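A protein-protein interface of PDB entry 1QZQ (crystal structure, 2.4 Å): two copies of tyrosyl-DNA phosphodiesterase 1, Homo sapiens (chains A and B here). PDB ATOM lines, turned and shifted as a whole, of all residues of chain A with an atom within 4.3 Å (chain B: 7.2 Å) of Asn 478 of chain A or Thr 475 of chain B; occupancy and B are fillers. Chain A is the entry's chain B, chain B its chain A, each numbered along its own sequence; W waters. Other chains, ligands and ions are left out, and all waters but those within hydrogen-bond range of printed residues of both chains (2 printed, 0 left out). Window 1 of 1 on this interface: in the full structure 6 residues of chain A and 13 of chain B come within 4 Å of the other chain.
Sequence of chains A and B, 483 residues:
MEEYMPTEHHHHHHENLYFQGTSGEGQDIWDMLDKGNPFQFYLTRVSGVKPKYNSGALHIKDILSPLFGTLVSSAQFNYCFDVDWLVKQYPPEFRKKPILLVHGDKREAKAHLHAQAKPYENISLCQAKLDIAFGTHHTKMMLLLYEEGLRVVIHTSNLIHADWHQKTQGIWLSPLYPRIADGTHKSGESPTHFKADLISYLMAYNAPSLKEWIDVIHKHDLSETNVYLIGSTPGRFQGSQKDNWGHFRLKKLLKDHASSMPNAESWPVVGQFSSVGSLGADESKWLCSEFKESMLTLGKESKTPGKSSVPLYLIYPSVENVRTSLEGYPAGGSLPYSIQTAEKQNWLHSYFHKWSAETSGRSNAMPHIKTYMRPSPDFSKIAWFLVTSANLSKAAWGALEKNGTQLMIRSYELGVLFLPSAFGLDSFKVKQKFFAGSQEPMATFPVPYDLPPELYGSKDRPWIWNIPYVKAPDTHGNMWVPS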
ATOM      1  N   TYR A 329      12.892  -6.103 -22.673  1.00  0.00           N
ATOM      2  CA  TYR A 329      13.044  -7.554 -22.617  1.00  0.00           C
ATOM      3  C   TYR A 329      13.124  -8.158 -21.204  1.00  0.00           C
ATOM      4  O   TYR A 329      12.620  -9.263 -20.966  1.00  0.00           O
ATOM      5  CB  TYR A 329      14.280  -7.979 -23.385  1.00  0.00           C
ATOM      6  CG  TYR A 329      14.155  -7.795 -24.868  1.00  0.00           C
ATOM      7  CD1 TYR A 329      13.200  -8.500 -25.590  1.00  0.00           C
ATOM      8  CD2 TYR A 329      15.022  -6.951 -25.560  1.00  0.00           C
ATOM      9  CE1 TYR A 329      13.116  -8.382 -26.960  1.00  0.00           C
ATOM     10  CE2 TYR A 329      14.942  -6.822 -26.932  1.00  0.00           C
ATOM     11  CZ  TYR A 329      13.991  -7.546 -27.634  1.00  0.00           C
ATOM     12  OH  TYR A 329      13.942  -7.474 -29.011  1.00  0.00           O
ATOM     13  N   PRO A 330      13.774  -7.455 -20.257  1.00  0.00           N
ATOM     14  CA  PRO A 330      13.861  -8.022 -18.908  1.00  0.00           C
ATOM     15  C   PRO A 330      12.513  -8.421 -18.322  1.00  0.00           C
ATOM     16  O   PRO A 330      12.468  -9.234 -17.394  1.00  0.00           O
ATOM     17  CB  PRO A 330      14.563  -6.917 -18.112  1.00  0.00           C
ATOM     18  CG  PRO A 330      15.512  -6.344 -19.143  1.00  0.00           C
ATOM     19  CD  PRO A 330      14.593  -6.231 -20.361  1.00  0.00           C
ATOM     20  N   PRO A 473      16.269  -3.848 -30.840  1.00  0.00           N
ATOM     21  CA  PRO A 473      16.513  -3.434 -29.455  1.00  0.00           C
ATOM     22  C   PRO A 473      15.203  -3.116 -28.738  1.00  0.00           C
ATOM     23  O   PRO A 473      14.235  -2.713 -29.376  1.00  0.00           O
ATOM     24  CB  PRO A 473      17.412  -2.208 -29.618  1.00  0.00           C
ATOM     25  CG  PRO A 473      16.898  -1.606 -30.920  1.00  0.00           C
ATOM     26  CD  PRO A 473      16.788  -2.851 -31.795  1.00  0.00           C
ATOM     27  N   ASP A 474      15.164  -3.290 -27.419  1.00  0.00           N
ATOM     28  CA  ASP A 474      13.928  -3.007 -26.697  1.00  0.00           C
ATOM     29  C   ASP A 474      13.801  -1.527 -26.360  1.00  0.00           C
ATOM     30  O   ASP A 474      14.585  -0.708 -26.843  1.00  0.00           O
ATOM     31  CB  ASP A 474      13.807  -3.880 -25.438  1.00  0.00           C
ATOM     32  CG  ASP A 474      14.771  -3.479 -24.320  1.00  0.00           C
ATOM     33  OD1 ASP A 474      14.814  -4.223 -23.321  1.00  0.00           O
ATOM     34  OD2 ASP A 474      15.469  -2.443 -24.417  1.00  0.00           O
ATOM     35  N   HIS A 476      14.708   0.132 -24.002  1.00  0.00           N
ATOM     36  CA  HIS A 476      15.869   0.730 -23.337  1.00  0.00           C
ATOM     37  C   HIS A 476      17.145   0.581 -24.173  1.00  0.00           C
ATOM     38  O   HIS A 476      18.247   0.725 -23.656  1.00  0.00           O
ATOM     39  CB  HIS A 476      16.077   0.078 -21.975  1.00  0.00           C
ATOM     40  CG  HIS A 476      14.917   0.239 -21.055  1.00  0.00           C
ATOM     41  ND1 HIS A 476      14.521   1.465 -20.568  1.00  0.00           N
ATOM     42  CD2 HIS A 476      14.065  -0.670 -20.525  1.00  0.00           C
ATOM     43  CE1 HIS A 476      13.477   1.305 -19.776  1.00  0.00           C
ATOM     44  NE2 HIS A 476      13.181   0.018 -19.734  1.00  0.00           N
ATOM     45  N   GLY A 477      16.975   0.262 -25.453  1.00  0.00           N
ATOM     46  CA  GLY A 477      18.099   0.103 -26.352  1.00  0.00           C
ATOM     47  C   GLY A 477      18.905  -1.174 -26.165  1.00  0.00           C
ATOM     48  O   GLY A 477      20.025  -1.286 -26.681  1.00  0.00           O
ATOM     49  N   ASN A 478      18.339  -2.143 -25.449  1.00  0.00           N
ATOM     50  CA  ASN A 478      19.026  -3.396 -25.195  1.00  0.00           C
ATOM     51  C   ASN A 478      18.487  -4.585 -25.962  1.00  0.00           C
ATOM     52  O   ASN A 478      17.385  -4.573 -26.517  1.00  0.00           O
ATOM     53  CB  ASN A 478      18.977  -3.750 -23.709  1.00  0.00           C
ATOM     54  CG  ASN A 478      19.577  -2.681 -22.832  1.00  0.00           C
ATOM     55  OD1 ASN A 478      20.702  -2.238 -23.055  1.00  0.00           O
ATOM     56  ND2 ASN A 478      18.832  -2.263 -21.817  1.00  0.00           N
ATOM     57  N   MET A 479      19.291  -5.636 -25.959  1.00  0.00           N
ATOM     58  CA  MET A 479      18.930  -6.873 -26.608  1.00  0.00           C
ATOM     59  C   MET A 479      18.803  -7.941 -25.537  1.00  0.00           C
ATOM     60  O   MET A 479      19.186  -7.728 -24.387  1.00  0.00           O
ATOM     61  CB  MET A 479      19.987  -7.230 -27.632  1.00  0.00           C
ATOM     62  CG  MET A 479      20.056  -6.185 -28.718  1.00  0.00           C
ATOM     63  SD  MET A 479      21.367  -6.597 -29.806  1.00  0.00           S
ATOM     64  CE  MET A 479      22.843  -5.787 -28.987  1.00  0.00           C
ATOM     65  N   TRP A 480      18.248  -9.084 -25.912  1.00  0.00           N
ATOM     66  CA  TRP A 480      18.042 -10.147 -24.956  1.00  0.00           C
ATOM     67  C   TRP A 480      18.883 -11.339 -25.335  1.00  0.00           C
ATOM     68  O   TRP A 480      18.702 -11.920 -26.408  1.00  0.00           O
ATOM     69  CB  TRP A 480      16.552 -10.530 -24.912  1.00  0.00           C
ATOM     70  CG  TRP A 480      16.208 -11.572 -23.871  1.00  0.00           C
ATOM     71  CD1 TRP A 480      15.832 -12.863 -24.100  1.00  0.00           C
ATOM     72  CD2 TRP A 480      16.132 -11.381 -22.448  1.00  0.00           C
ATOM     73  NE1 TRP A 480      15.515 -13.481 -22.915  1.00  0.00           N
ATOM     74  CE2 TRP A 480      15.691 -12.593 -21.888  1.00  0.00           C
ATOM     75  CE3 TRP A 480      16.393 -10.301 -21.597  1.00  0.00           C
ATOM     76  CZ2 TRP A 480      15.498 -12.756 -20.517  1.00  0.00           C
ATOM     77  CZ3 TRP A 480      16.203 -10.466 -20.235  1.00  0.00           C
ATOM     78  CH2 TRP A 480      15.759 -11.685 -19.711  1.00  0.00           C
ATOM     79  N   GLU B 320      27.789   3.638 -21.534  1.00  0.00           N
ATOM     80  CA  GLU B 320      26.835   3.008 -22.441  1.00  0.00           C
ATOM     81  C   GLU B 320      27.316   1.647 -22.993  1.00  0.00           C
ATOM     82  O   GLU B 320      26.490   0.770 -23.278  1.00  0.00           O
ATOM     83  CB  GLU B 320      26.513   3.952 -23.602  1.00  0.00           C
ATOM     84  CG  GLU B 320      25.330   3.515 -24.420  1.00  0.00           C
ATOM     85  CD  GLU B 320      23.998   3.671 -23.675  1.00  0.00           C
ATOM     86  OE1 GLU B 320      23.995   3.952 -22.445  1.00  0.00           O
ATOM     87  OE2 GLU B 320      22.949   3.500 -24.338  1.00  0.00           O
ATOM     88  N   VAL B 322      29.038  -0.504 -21.346  1.00  0.00           N
ATOM     89  CA  VAL B 322      28.779  -1.385 -20.209  1.00  0.00           C
ATOM     90  C   VAL B 322      27.306  -1.645 -19.944  1.00  0.00           C
ATOM     91  O   VAL B 322      26.909  -2.781 -19.666  1.00  0.00           O
ATOM     92  CB  VAL B 322      29.408  -0.815 -18.904  1.00  0.00           C
ATOM     93  CG1 VAL B 322      29.019  -1.689 -17.708  1.00  0.00           C
ATOM     94  CG2 VAL B 322      30.920  -0.755 -19.037  1.00  0.00           C
ATOM     95  N   ARG B 323      26.499  -0.595 -20.022  1.00  0.00           N
ATOM     96  CA  ARG B 323      25.073  -0.746 -19.778  1.00  0.00           C
ATOM     97  C   ARG B 323      24.478  -1.754 -20.744  1.00  0.00           C
ATOM     98  O   ARG B 323      23.685  -2.610 -20.363  1.00  0.00           O
ATOM     99  CB  ARG B 323      24.324   0.590 -19.943  1.00  0.00           C
ATOM    100  CG  ARG B 323      22.806   0.482 -19.657  1.00  0.00           C
ATOM    101  CD  ARG B 323      22.062   1.804 -19.833  1.00  0.00           C
ATOM    102  NE  ARG B 323      21.841   2.140 -21.239  1.00  0.00           N
ATOM    103  CZ  ARG B 323      20.842   1.668 -21.984  1.00  0.00           C
ATOM    104  NH1 ARG B 323      19.950   0.837 -21.466  1.00  0.00           N
ATOM    105  NH2 ARG B 323      20.741   2.015 -23.259  1.00  0.00           N
ATOM    106  N   THR B 324      24.866  -1.655 -22.003  1.00  0.00           N
ATOM    107  CA  THR B 324      24.305  -2.538 -23.010  1.00  0.00           C
ATOM    108  C   THR B 324      25.057  -3.859 -23.197  1.00  0.00           C
ATOM    109  O   THR B 324      24.736  -4.636 -24.095  1.00  0.00           O
ATOM    110  CB  THR B 324      24.245  -1.812 -24.362  1.00  0.00           C
ATOM    111  OG1 THR B 324      25.572  -1.434 -24.746  1.00  0.00           O
ATOM    112  CG2 THR B 324      23.380  -0.560 -24.254  1.00  0.00           C
ATOM    113  N   SER B 325      26.051  -4.112 -22.355  1.00  0.00           N
ATOM    114  CA  SER B 325      26.830  -5.321 -22.488  1.00  0.00           C
ATOM    115  C   SER B 325      26.041  -6.568 -22.104  1.00  0.00           C
ATOM    116  O   SER B 325      24.983  -6.488 -21.472  1.00  0.00           O
ATOM    117  CB  SER B 325      28.087  -5.231 -21.624  1.00  0.00           C
ATOM    118  OG  SER B 325      27.739  -5.315 -20.247  1.00  0.00           O
ATOM    119  N   LEU B 326      26.578  -7.719 -22.505  1.00  0.00           N
ATOM    120  CA  LEU B 326      25.969  -9.000 -22.211  1.00  0.00           C
ATOM    121  C   LEU B 326      25.791  -9.127 -20.695  1.00  0.00           C
ATOM    122  O   LEU B 326      24.788  -9.666 -20.238  1.00  0.00           O
ATOM    123  CB  LEU B 326      26.847 -10.147 -22.751  1.00  0.00           C
ATOM    124  CG  LEU B 326      26.965 -10.329 -24.271  1.00  0.00           C
ATOM    125  CD1 LEU B 326      27.978 -11.432 -24.614  1.00  0.00           C
ATOM    126  CD2 LEU B 326      25.616 -10.711 -24.831  1.00  0.00           C
ATOM    127  N   GLU B 327      26.749  -8.617 -19.919  1.00  0.00           N
ATOM    128  CA  GLU B 327      26.654  -8.699 -18.454  1.00  0.00           C
ATOM    129  C   GLU B 327      25.871  -7.573 -17.795  1.00  0.00           C
ATOM    130  O   GLU B 327      25.377  -7.716 -16.674  1.00  0.00           O
ATOM    131  CB  GLU B 327      28.032  -8.679 -17.813  1.00  0.00           C
ATOM    132  CG  GLU B 327      28.910  -9.853 -18.100  1.00  0.00           C
ATOM    133  CD  GLU B 327      30.260  -9.670 -17.444  1.00  0.00           C
ATOM    134  OE1 GLU B 327      30.371  -9.927 -16.213  1.00  0.00           O
ATOM    135  OE2 GLU B 327      31.194  -9.241 -18.161  1.00  0.00           O
ATOM    136  N   GLY B 328      25.793  -6.443 -18.480  1.00  0.00           N
ATOM    137  CA  GLY B 328      25.120  -5.289 -17.914  1.00  0.00           C
ATOM    138  C   GLY B 328      26.102  -4.578 -17.004  1.00  0.00           C
ATOM    139  O   GLY B 328      27.303  -4.759 -17.138  1.00  0.00           O
ATOM    140  N   TYR B 329      25.603  -3.795 -16.056  1.00  0.00           N
ATOM    141  CA  TYR B 329      26.478  -3.067 -15.146  1.00  0.00           C
ATOM    142  C   TYR B 329      27.507  -3.934 -14.408  1.00  0.00           C
ATOM    143  O   TYR B 329      28.614  -3.479 -14.139  1.00  0.00           O
ATOM    144  CB  TYR B 329      25.644  -2.244 -14.147  1.00  0.00           C
ATOM    145  CG  TYR B 329      24.914  -1.079 -14.796  1.00  0.00           C
ATOM    146  CD1 TYR B 329      25.611  -0.097 -15.507  1.00  0.00           C
ATOM    147  CD2 TYR B 329      23.528  -0.971 -14.718  1.00  0.00           C
ATOM    148  CE1 TYR B 329      24.943   0.961 -16.123  1.00  0.00           C
ATOM    149  CE2 TYR B 329      22.846   0.084 -15.330  1.00  0.00           C
ATOM    150  CZ  TYR B 329      23.555   1.045 -16.028  1.00  0.00           C
ATOM    151  OH  TYR B 329      22.868   2.086 -16.616  1.00  0.00           O
ATOM    152  N   PRO B 330      27.167  -5.194 -14.086  1.00  0.00           N
ATOM    153  CA  PRO B 330      28.134  -6.050 -13.383  1.00  0.00           C
ATOM    154  C   PRO B 330      29.491  -6.165 -14.086  1.00  0.00           C
ATOM    155  O   PRO B 330      30.516  -6.450 -13.439  1.00  0.00           O
ATOM    156  CB  PRO B 330      27.399  -7.380 -13.283  1.00  0.00           C
ATOM    157  CG  PRO B 330      25.979  -6.920 -13.067  1.00  0.00           C
ATOM    158  CD  PRO B 330      25.846  -5.843 -14.140  1.00  0.00           C
ATOM    159  N   ASN B 364      29.547  -6.438 -27.466  1.00  0.00           N
ATOM    160  CA  ASN B 364      28.840  -6.498 -26.183  1.00  0.00           C
ATOM    161  C   ASN B 364      29.544  -7.316 -25.100  1.00  0.00           C
ATOM    162  O   ASN B 364      29.025  -7.463 -23.983  1.00  0.00           O
ATOM    163  CB  ASN B 364      27.416  -7.026 -26.400  1.00  0.00           C
ATOM    164  CG  ASN B 364      26.608  -6.147 -27.353  1.00  0.00           C
ATOM    165  OD1 ASN B 364      26.201  -5.038 -27.003  1.00  0.00           O
ATOM    166  ND2 ASN B 364      26.397  -6.636 -28.565  1.00  0.00           N
ATOM    167  N   ALA B 472      19.224   4.792 -16.839  1.00  0.00           N
ATOM    168  CA  ALA B 472      18.752   3.742 -17.734  1.00  0.00           C
ATOM    169  C   ALA B 472      19.210   2.378 -17.224  1.00  0.00           C
ATOM    170  O   ALA B 472      20.334   2.220 -16.762  1.00  0.00           O
ATOM    171  CB  ALA B 472      19.270   3.995 -19.151  1.00  0.00           C
ATOM    172  N   PRO B 473      18.333   1.375 -17.303  1.00  0.00           N
ATOM    173  CA  PRO B 473      18.618   0.014 -16.848  1.00  0.00           C
ATOM    174  C   PRO B 473      19.494  -0.766 -17.824  1.00  0.00           C
ATOM    175  O   PRO B 473      19.587  -0.413 -19.003  1.00  0.00           O
ATOM    176  CB  PRO B 473      17.224  -0.588 -16.699  1.00  0.00           C
ATOM    177  CG  PRO B 473      16.499   0.020 -17.873  1.00  0.00           C
ATOM    178  CD  PRO B 473      16.960   1.478 -17.832  1.00  0.00           C
ATOM    179  N   ASP B 474      20.113  -1.837 -17.332  1.00  0.00           N
ATOM    180  CA  ASP B 474      20.982  -2.632 -18.169  1.00  0.00           C
ATOM    181  C   ASP B 474      20.254  -3.794 -18.817  1.00  0.00           C
ATOM    182  O   ASP B 474      19.023  -3.935 -18.701  1.00  0.00           O
ATOM    183  CB  ASP B 474      22.196  -3.123 -17.365  1.00  0.00           C
ATOM    184  CG  ASP B 474      21.836  -4.152 -16.298  1.00  0.00           C
ATOM    185  OD1 ASP B 474      22.739  -4.459 -15.490  1.00  0.00           O
ATOM    186  OD2 ASP B 474      20.687  -4.666 -16.263  1.00  0.00           O
ATOM    187  N   THR B 475      21.018  -4.627 -19.511  1.00  0.00           N
ATOM    188  CA  THR B 475      20.440  -5.756 -20.206  1.00  0.00           C
ATOM    189  C   THR B 475      19.711  -6.743 -19.299  1.00  0.00           C
ATOM    190  O   THR B 475      19.059  -7.654 -19.783  1.00  0.00           O
ATOM    191  CB  THR B 475      21.512  -6.487 -20.994  1.00  0.00           C
ATOM    192  OG1 THR B 475      22.581  -6.849 -20.114  1.00  0.00           O
ATOM    193  CG2 THR B 475      22.051  -5.594 -22.105  1.00  0.00           C
ATOM    194  N   HIS B 476      19.818  -6.572 -17.986  1.00  0.00           N
ATOM    195  CA  HIS B 476      19.129  -7.485 -17.069  1.00  0.00           C
ATOM    196  C   HIS B 476      18.038  -6.774 -16.270  1.00  0.00           C
ATOM    197  O   HIS B 476      17.474  -7.350 -15.345  1.00  0.00           O
ATOM    198  CB  HIS B 476      20.128  -8.146 -16.117  1.00  0.00           C
ATOM    199  CG  HIS B 476      21.150  -8.989 -16.817  1.00  0.00           C
ATOM    200  ND1 HIS B 476      20.849 -10.212 -17.378  1.00  0.00           N
ATOM    201  CD2 HIS B 476      22.455  -8.759 -17.096  1.00  0.00           C
ATOM    202  CE1 HIS B 476      21.924 -10.696 -17.973  1.00  0.00           C
ATOM    203  NE2 HIS B 476      22.910  -9.834 -17.817  1.00  0.00           N
ATOM    204  N   GLY B 477      17.749  -5.528 -16.653  1.00  0.00           N
ATOM    205  CA  GLY B 477      16.736  -4.741 -15.982  1.00  0.00           C
ATOM    206  C   GLY B 477      17.219  -4.051 -14.721  1.00  0.00           C
ATOM    207  O   GLY B 477      16.424  -3.423 -14.025  1.00  0.00           O
ATOM    208  N   ASN B 478      18.514  -4.126 -14.437  1.00  0.00           N
ATOM    209  CA  ASN B 478      19.059  -3.516 -13.229  1.00  0.00           C
ATOM    210  C   ASN B 478      19.773  -2.195 -13.391  1.00  0.00           C
ATOM    211  O   ASN B 478      20.127  -1.789 -14.501  1.00  0.00           O
ATOM    212  CB  ASN B 478      20.025  -4.483 -12.557  1.00  0.00           C
ATOM    213  CG  ASN B 478      19.422  -5.842 -12.369  1.00  0.00           C
ATOM    214  OD1 ASN B 478      18.325  -5.976 -11.810  1.00  0.00           O
ATOM    215  ND2 ASN B 478      20.120  -6.864 -12.836  1.00  0.00           N
HETATM  216  O   HOH W   1      17.686  -6.498 -22.145  1.00  0.00           O
HETATM  217  O   HOH W   2      22.374  -4.832 -25.636  1.00  0.00           O
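The backbone carbonyl oxygen of His 476 of chain A sits at hydrogen-bond distance from the guanidinium group of Arg 323 of chain B, at 2.8 Å.
O of Pro 473 of chain B sits at hydrogen-bond distance from ND2 of Asn 478 of chain A (3.5 Å).
The side-chain amide nitrogen (ND2) of Asn 478 of chain A lies close to the guanidinium group (NH1) of Arg 323 of chain B, 3.3 Å away.
N of Gly 477 of chain B sits at hydrogen-bond distance from OD2 of Asp 474 of chain B (3.1 Å).
OD2 of Asp 474 of chain B sits at hydrogen-bond distance from N of His 476 of chain B (2.7 Å).
O of Glu 327 of chain B sits close to NE2 of His 476 of chain B, at 3.4 Å.
The backbone NH (N) of His 476 of chain A sits at hydrogen-bond distance from the side-chain carboxylate (OD2) of Asp 474 of chain A (2.7 Å).
N of Asn 478 of chain A lies within hydrogen-bond range of OD2 of Asp 474 of chain A, 3.1 Å away.
The backbone carbonyl oxygen (O) of Asn 364 of chain B is in hydrogen-bond range of the backbone NH (N) of Leu 326 of chain B, 2.9 Å away.
Pro 330 of chain A touches Thr 475 of chain B (CG to O, 3.8 Å).
His 476 of chain B touches Pro 330 of chain A.
CG of Pro 330 of chain A touches N of Gly 477 of chain B (3.4 Å).
CG of His 476 of chain A touches CG of Pro 473 of chain B (3.6 Å).
Thr 324 of chain B touches Asn 478 of chain A (CG2 to OD1, 3.4 Å).
Asp 474 of chain B touches Asn 478 of chain A.
OD1 of Asn 478 of chain A touches CG2 of Thr 475 of chain B, at 3.7 Å.
CE of Met 479 of chain A touches ND2 of Asn 364 of chain B, 3.7 Å away.
Asn 478 of chain A touches just these residues of chain B: Arg 323 (3.3 Å), Thr 324 (3.4 Å), Pro 473 (3.5 Å), Asp 474 (3.5 Å) and Thr 475 (3.7 Å).
Thr 475 of chain B touches two residues of chain A.
Gly 477 of chain A touches none of the printed residues of chain B.
Printed residues of chain A within 4 Å of Asn 364 of chain B: Met 479.
Of the printed residues of chain A, Thr 324 of chain B touches Asn 478 (3.4 Å).
Printed residues of chain A within 4 Å of Gly 477 of chain B: Pro 330 (3.4 Å).
Of the printed residues of chain B, Met 479 of chain A touches Asn 364.
Gly 328 of chain B touches none of the printed residues of chain A.
The nearest residue of chain B that does not touch Asn 478 of chain A is Ser 325 of chain B (5.7 Å).
Hydrophobic or aromatic side chains of chain A within 4 Å of the printed part of chain B: Pro 330, His 476 and Met 479.
Printed residues of chain B that touch a printed residue of chain A: Arg 323, Thr 324, Asn 364, Pro 473, Asp 474, Thr 475, His 476 and Gly 477.
Among the printed residues, no Asp or Glu carboxylate lies within 4 Å of a Lys or Arg side-chain nitrogen of the other chain.
Pro 330 of chain A touches His 476 of chain B, but with the chains exchanged His 476 of chain A does not touch Pro 330 of chain B (13.8 Å).
Pro 330 of chain A touches Gly 477 of chain B, but with the chains exchanged Gly 477 of chain A does not touch Pro 330 of chain B (14.6 Å).
Asn 478 of chain A touches Pro 473 of chain B, but with the chains exchanged Pro 473 of chain A does not touch Asn 478 of chain B (14.7 Å).
Asn 478 of chain A touches Asp 474 of chain B, but with the chains exchanged Asp 474 of chain A does not touch Asn 478 of chain B (9.6 Å).
Positions printed for both chains: 329, 330, 473, 474, 476, 477 and 478.
Water W2 bridges O of Thr 324 of chain B (2.8 Å) and N of Met 479 of chain A (3.2 Å).
Water W1 bridges O of Met 479 of chain A (3.0 Å) and O of Thr 475 of chain B (3.0 Å).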
